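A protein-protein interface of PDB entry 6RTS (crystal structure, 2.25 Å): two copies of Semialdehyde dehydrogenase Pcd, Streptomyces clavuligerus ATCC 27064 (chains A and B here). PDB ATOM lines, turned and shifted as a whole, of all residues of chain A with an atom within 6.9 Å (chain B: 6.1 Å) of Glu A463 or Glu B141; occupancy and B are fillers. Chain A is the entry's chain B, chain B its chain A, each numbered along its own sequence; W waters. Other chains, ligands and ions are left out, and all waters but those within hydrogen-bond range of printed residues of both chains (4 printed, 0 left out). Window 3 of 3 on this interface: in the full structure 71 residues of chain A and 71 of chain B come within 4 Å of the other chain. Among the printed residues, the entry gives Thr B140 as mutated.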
ATOM      1  N   GLU A 118      -2.463  21.997  16.170  1.00  0.00           N
ATOM      2  CA  GLU A 118      -2.464  20.996  17.240  1.00  0.00           C
ATOM      3  C   GLU A 118      -2.576  21.663  18.634  1.00  0.00           C
ATOM      4  O   GLU A 118      -3.321  21.197  19.508  1.00  0.00           O
ATOM      5  CB  GLU A 118      -1.177  20.162  17.108  1.00  0.00           C
ATOM      6  CG  GLU A 118      -1.026  19.002  18.056  1.00  0.00           C
ATOM      7  CD  GLU A 118      -1.588  17.697  17.544  1.00  0.00           C
ATOM      8  OE1 GLU A 118      -2.013  17.598  16.368  1.00  0.00           O
ATOM      9  OE2 GLU A 118      -1.579  16.745  18.349  1.00  0.00           O
ATOM     10  N   ASP A 121      -6.123  22.906  18.904  1.00  0.00           N
ATOM     11  CA  ASP A 121      -7.020  21.778  19.123  1.00  0.00           C
ATOM     12  C   ASP A 121      -6.951  21.198  20.550  1.00  0.00           C
ATOM     13  O   ASP A 121      -7.999  20.801  21.078  1.00  0.00           O
ATOM     14  CB  ASP A 121      -6.784  20.666  18.094  1.00  0.00           C
ATOM     15  CG  ASP A 121      -7.058  21.113  16.668  1.00  0.00           C
ATOM     16  OD1 ASP A 121      -7.782  22.110  16.482  1.00  0.00           O
ATOM     17  OD2 ASP A 121      -6.528  20.486  15.727  1.00  0.00           O
ATOM     18  N   SER A 460       2.607   7.637  11.769  1.00  0.00           N
ATOM     19  CA  SER A 460       2.196   8.956  12.286  1.00  0.00           C
ATOM     20  C   SER A 460       0.682   9.124  12.445  1.00  0.00           C
ATOM     21  O   SER A 460       0.220  10.197  12.818  1.00  0.00           O
ATOM     22  CB  SER A 460       2.772  10.074  11.422  1.00  0.00           C
ATOM     23  OG  SER A 460       4.186  10.055  11.526  1.00  0.00           O
ATOM     24  N   GLY A 461      -0.080   8.067  12.200  1.00  0.00           N
ATOM     25  CA  GLY A 461      -1.526   8.082  12.388  1.00  0.00           C
ATOM     26  C   GLY A 461      -1.927   8.177  13.845  1.00  0.00           C
ATOM     27  O   GLY A 461      -2.091   7.179  14.533  1.00  0.00           O
ATOM     28  N   ALA A 462      -2.072   9.399  14.307  1.00  0.00           N
ATOM     29  CA  ALA A 462      -2.475   9.655  15.663  1.00  0.00           C
ATOM     30  C   ALA A 462      -3.145  11.027  15.697  1.00  0.00           C
ATOM     31  O   ALA A 462      -2.979  11.809  14.765  1.00  0.00           O
ATOM     32  CB  ALA A 462      -1.251   9.596  16.553  1.00  0.00           C
ATOM     33  N   GLU A 463      -3.906  11.310  16.753  1.00  0.00           N
ATOM     34  CA  GLU A 463      -4.673  12.572  16.863  1.00  0.00           C
ATOM     35  C   GLU A 463      -5.025  12.962  18.321  1.00  0.00           C
ATOM     36  O   GLU A 463      -4.877  12.160  19.243  1.00  0.00           O
ATOM     37  CB  GLU A 463      -5.941  12.483  16.017  1.00  0.00           C
ATOM     38  CG  GLU A 463      -6.980  11.452  16.470  1.00  0.00           C
ATOM     39  CD  GLU A 463      -8.136  11.383  15.470  1.00  0.00           C
ATOM     40  OE1 GLU A 463      -9.051  12.241  15.542  1.00  0.00           O
ATOM     41  OE2 GLU A 463      -8.107  10.490  14.593  1.00  0.00           O
ATOM     42  N   ILE A 464      -5.497  14.197  18.503  1.00  0.00           N
ATOM     43  CA  ILE A 464      -5.659  14.814  19.840  1.00  0.00           C
ATOM     44  C   ILE A 464      -6.443  13.946  20.810  1.00  0.00           C
ATOM     45  O   ILE A 464      -6.047  13.773  21.964  1.00  0.00           O
ATOM     46  CB  ILE A 464      -6.337  16.224  19.722  1.00  0.00           C
ATOM     47  CG1 ILE A 464      -5.363  17.250  19.134  1.00  0.00           C
ATOM     48  CG2 ILE A 464      -6.857  16.747  21.055  1.00  0.00           C
ATOM     49  CD1 ILE A 464      -4.077  17.467  19.922  1.00  0.00           C
ATOM     50  N   GLY A 465      -7.552  13.407  20.324  1.00  0.00           N
ATOM     51  CA  GLY A 465      -8.442  12.595  21.141  1.00  0.00           C
ATOM     52  C   GLY A 465      -7.914  11.253  21.606  1.00  0.00           C
ATOM     53  O   GLY A 465      -8.471  10.667  22.538  1.00  0.00           O
ATOM     54  N   GLY A 466      -6.873  10.758  20.938  1.00  0.00           N
ATOM     55  CA  GLY A 466      -6.131   9.578  21.382  1.00  0.00           C
ATOM     56  C   GLY A 466      -5.042   9.920  22.401  1.00  0.00           C
ATOM     57  O   GLY A 466      -4.413  10.954  22.291  1.00  0.00           O
ATOM     58  N   ALA A 467      -4.850   9.056  23.402  1.00  0.00           N
ATOM     59  CA  ALA A 467      -3.688   9.115  24.288  1.00  0.00           C
ATOM     60  C   ALA A 467      -2.425   8.789  23.463  1.00  0.00           C
ATOM     61  O   ALA A 467      -2.394   7.791  22.692  1.00  0.00           O
ATOM     62  CB  ALA A 467      -3.847   8.134  25.454  1.00  0.00           C
ATOM     63  N   PHE A 468      -1.409   9.649  23.590  1.00  0.00           N
ATOM     64  CA  PHE A 468      -0.206   9.542  22.770  1.00  0.00           C
ATOM     65  C   PHE A 468       1.035   9.091  23.557  1.00  0.00           C
ATOM     66  O   PHE A 468       1.429   9.729  24.526  1.00  0.00           O
ATOM     67  CB  PHE A 468       0.070  10.867  22.104  1.00  0.00           C
ATOM     68  CG  PHE A 468       1.284  10.840  21.244  1.00  0.00           C
ATOM     69  CD1 PHE A 468       2.528  11.132  21.778  1.00  0.00           C
ATOM     70  CD2 PHE A 468       1.192  10.447  19.910  1.00  0.00           C
ATOM     71  CE1 PHE A 468       3.649  11.078  20.990  1.00  0.00           C
ATOM     72  CE2 PHE A 468       2.315  10.397  19.110  1.00  0.00           C
ATOM     73  CZ  PHE A 468       3.549  10.723  19.654  1.00  0.00           C
ATOM     74  N   GLU A 479       0.284  11.236  26.692  1.00  0.00           N
ATOM     75  CA  GLU A 479      -0.094  12.636  26.651  1.00  0.00           C
ATOM     76  C   GLU A 479      -1.330  12.846  25.798  1.00  0.00           C
ATOM     77  O   GLU A 479      -1.707  11.989  25.010  1.00  0.00           O
ATOM     78  CB  GLU A 479       1.045  13.454  26.061  1.00  0.00           C
ATOM     79  CG  GLU A 479       2.300  13.443  26.912  1.00  0.00           C
ATOM     80  CD  GLU A 479       3.490  14.021  26.190  1.00  0.00           C
ATOM     81  OE1 GLU A 479       4.189  14.858  26.782  1.00  0.00           O
ATOM     82  OE2 GLU A 479       3.723  13.640  25.022  1.00  0.00           O
ATOM     83  N   SER A 480      -1.916  14.029  25.947  1.00  0.00           N
ATOM     84  CA  SER A 480      -2.991  14.534  25.074  1.00  0.00           C
ATOM     85  C   SER A 480      -4.363  13.913  25.394  1.00  0.00           C
ATOM     86  O   SER A 480      -5.021  14.371  26.324  1.00  0.00           O
ATOM     87  CB  SER A 480      -2.624  14.419  23.581  1.00  0.00           C
ATOM     88  OG  SER A 480      -3.567  15.123  22.768  1.00  0.00           O
ATOM     89  N   GLY A 481      -4.761  12.857  24.677  1.00  0.00           N
ATOM     90  CA  GLY A 481      -6.153  12.422  24.633  1.00  0.00           C
ATOM     91  C   GLY A 481      -6.622  11.436  25.685  1.00  0.00           C
ATOM     92  O   GLY A 481      -5.910  11.166  26.669  1.00  0.00           O
ATOM     93  N   PRO B 139     -14.677   9.231  18.431  1.00  0.00           N
ATOM     94  CA  PRO B 139     -14.594   9.747  17.068  1.00  0.00           C
ATOM     95  C   PRO B 139     -13.160  10.070  16.654  1.00  0.00           C
ATOM     96  O   PRO B 139     -12.331  10.401  17.504  1.00  0.00           O
ATOM     97  CB  PRO B 139     -15.425  11.041  17.118  1.00  0.00           C
ATOM     98  CG  PRO B 139     -16.274  10.930  18.327  1.00  0.00           C
ATOM     99  CD  PRO B 139     -15.506  10.093  19.296  1.00  0.00           C
ATOM    100  N   THR B 140     -12.915   9.975  15.350  1.00  0.00           N
ATOM    101  CA  THR B 140     -11.673  10.411  14.724  1.00  0.00           C
ATOM    102  C   THR B 140     -11.983  11.576  13.792  1.00  0.00           C
ATOM    103  O   THR B 140     -13.009  11.565  13.118  1.00  0.00           O
ATOM    104  CB  THR B 140     -10.987   9.298  13.884  1.00  0.00           C
ATOM    105  OG1 THR B 140      -9.955   9.870  13.076  1.00  0.00           O
ATOM    106  CG2 THR B 140     -11.944   8.589  12.945  1.00  0.00           C
ATOM    107  N   GLU B 141     -11.075  12.542  13.721  1.00  0.00           N
ATOM    108  CA  GLU B 141     -11.161  13.619  12.740  1.00  0.00           C
ATOM    109  C   GLU B 141     -11.029  13.155  11.275  1.00  0.00           C
ATOM    110  O   GLU B 141     -11.315  13.919  10.373  1.00  0.00           O
ATOM    111  CB  GLU B 141     -10.101  14.689  13.031  1.00  0.00           C
ATOM    112  CG  GLU B 141      -8.684  14.224  12.732  1.00  0.00           C
ATOM    113  CD  GLU B 141      -7.580  15.102  13.315  1.00  0.00           C
ATOM    114  OE1 GLU B 141      -7.809  15.806  14.350  1.00  0.00           O
ATOM    115  OE2 GLU B 141      -6.451  15.026  12.734  1.00  0.00           O
ATOM    116  N   ARG B 142     -10.593  11.924  11.043  1.00  0.00           N
ATOM    117  CA  ARG B 142     -10.311  11.414   9.701  1.00  0.00           C
ATOM    118  C   ARG B 142     -11.573  10.758   9.097  1.00  0.00           C
ATOM    119  O   ARG B 142     -12.100   9.807   9.674  1.00  0.00           O
ATOM    120  CB  ARG B 142      -9.173  10.373   9.772  1.00  0.00           C
ATOM    121  CG  ARG B 142      -7.886  10.846  10.441  1.00  0.00           C
ATOM    122  CD  ARG B 142      -6.877   9.706  10.557  1.00  0.00           C
ATOM    123  NE  ARG B 142      -5.751  10.065  11.425  1.00  0.00           N
ATOM    124  CZ  ARG B 142      -4.738  10.870  11.090  1.00  0.00           C
ATOM    125  NH1 ARG B 142      -4.663  11.428   9.882  1.00  0.00           N
ATOM    126  NH2 ARG B 142      -3.780  11.115  11.981  1.00  0.00           N
ATOM    127  N   PRO B 143     -12.074  11.270   7.947  1.00  0.00           N
ATOM    128  CA  PRO B 143     -13.211  10.629   7.272  1.00  0.00           C
ATOM    129  C   PRO B 143     -12.907   9.201   6.847  1.00  0.00           C
ATOM    130  O   PRO B 143     -11.792   8.917   6.379  1.00  0.00           O
ATOM    131  CB  PRO B 143     -13.426  11.484   6.016  1.00  0.00           C
ATOM    132  CG  PRO B 143     -12.617  12.709   6.181  1.00  0.00           C
ATOM    133  CD  PRO B 143     -11.572  12.448   7.215  1.00  0.00           C
ATOM    134  N   LEU B 147     -11.559   5.026  15.440  1.00  0.00           N
ATOM    135  CA  LEU B 147     -10.543   5.207  16.486  1.00  0.00           C
ATOM    136  C   LEU B 147     -11.007   4.526  17.768  1.00  0.00           C
ATOM    137  O   LEU B 147     -12.176   4.609  18.133  1.00  0.00           O
ATOM    138  CB  LEU B 147     -10.274   6.696  16.761  1.00  0.00           C
ATOM    139  CG  LEU B 147      -9.274   7.126  17.862  1.00  0.00           C
ATOM    140  CD1 LEU B 147      -7.871   6.557  17.683  1.00  0.00           C
ATOM    141  CD2 LEU B 147      -9.158   8.634  17.905  1.00  0.00           C
ATOM    142  N   THR B 495      -6.087   3.474  15.276  1.00  0.00           N
ATOM    143  CA  THR B 495      -6.787   4.105  14.180  1.00  0.00           C
ATOM    144  C   THR B 495      -6.873   3.104  13.038  1.00  0.00           C
ATOM    145  O   THR B 495      -5.860   2.543  12.613  1.00  0.00           O
ATOM    146  CB  THR B 495      -6.066   5.361  13.686  1.00  0.00           C
ATOM    147  OG1 THR B 495      -5.927   6.298  14.757  1.00  0.00           O
ATOM    148  CG2 THR B 495      -6.825   6.045  12.512  1.00  0.00           C
HETATM  149  O   HOH W   1      -5.087  15.895  15.896  1.00  0.00           O
HETATM  150  O   HOH W   2      -3.736  14.514  13.660  1.00  0.00           O
HETATM  151  O   HOH W   3      -5.731   9.239  14.231  1.00  0.00           O
HETATM  152  O   HOH W   4      -3.794   5.950  16.454  1.00  0.00           O
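The backbone NH (N) of Glu B141 is in hydrogen-bond range of the side-chain carboxylate (OE1) of Glu A463 (2.7 Å).
The guanidinium group (NH2) of Arg B142 is in hydrogen-bond range of the backbone carbonyl oxygen (O) of Ala A462.
The side-chain carboxylate of Glu A463 is in salt-bridge range of the guanidinium group of Arg B142.
OG1 of Thr B140 is in hydrogen-bond range of OE2 of Glu A463.
OG1 of Thr B140 is in hydrogen-bond range of N of Arg B142, at 3.0 Å.
Among the printed residues, pairs that only touch across the chains: Gly A461 with Arg B142, Gly A461 with Thr B495 and Glu A463 with Leu B147.
Of the printed residues of chain B, Gly A461 touches Arg B142 and Thr B495.
Of the printed residues of chain B, Ala A462 touches Arg B142 (3.0 Å).
Glu A463 touches four residues of chain B.
Printed residues of chain A within 4 Å of Thr B140: Glu A463 (2.5 Å).
Glu B141 touches just one residue of chain A: Glu A463 (2.7 Å).
Of the printed residues of chain A, Arg B142 touches Gly A461, Ala A462 and Glu A463.
Of the printed residues of chain A, Leu B147 touches Glu A463.
The nearest printed residue of chain A that does not touch Glu B141 is Ile A464 (5.0 Å).
The nearest printed residue of chain A that does not touch Leu B147 is Gly A466 (4.4 Å).
Of the 14 printed residues of chain A, 3 touch a printed residue of chain B.
Among the printed residues, 7 pairs touch across the chains.
Among the printed residues, Asp or Glu carboxylates within 4 Å of a Lys or Arg side-chain nitrogen of the other chain: Glu A463 with Arg B142.
No position is printed for both chains.
Of the 7 pairs that touch across the chains among the printed residues, none has its exchanged pair printed and touching as well.
Water W3 lies within hydrogen-bond range of the side-chain carboxylate of Glu A463, the guanidinium group of Arg B142 and the side-chain hydroxyl of Thr B495.
Water W4 bridges OG1 of Thr B495 and O of Gly A461.
Water W2 lies within hydrogen-bond range of OE2 of Glu B141 and O of Ala A462.
Water W1 lies within hydrogen-bond range of the side-chain carboxylate (OE1) of Glu B141 (3.1 Å) and the backbone NH (N) of Ile A464 (3.1 Å).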
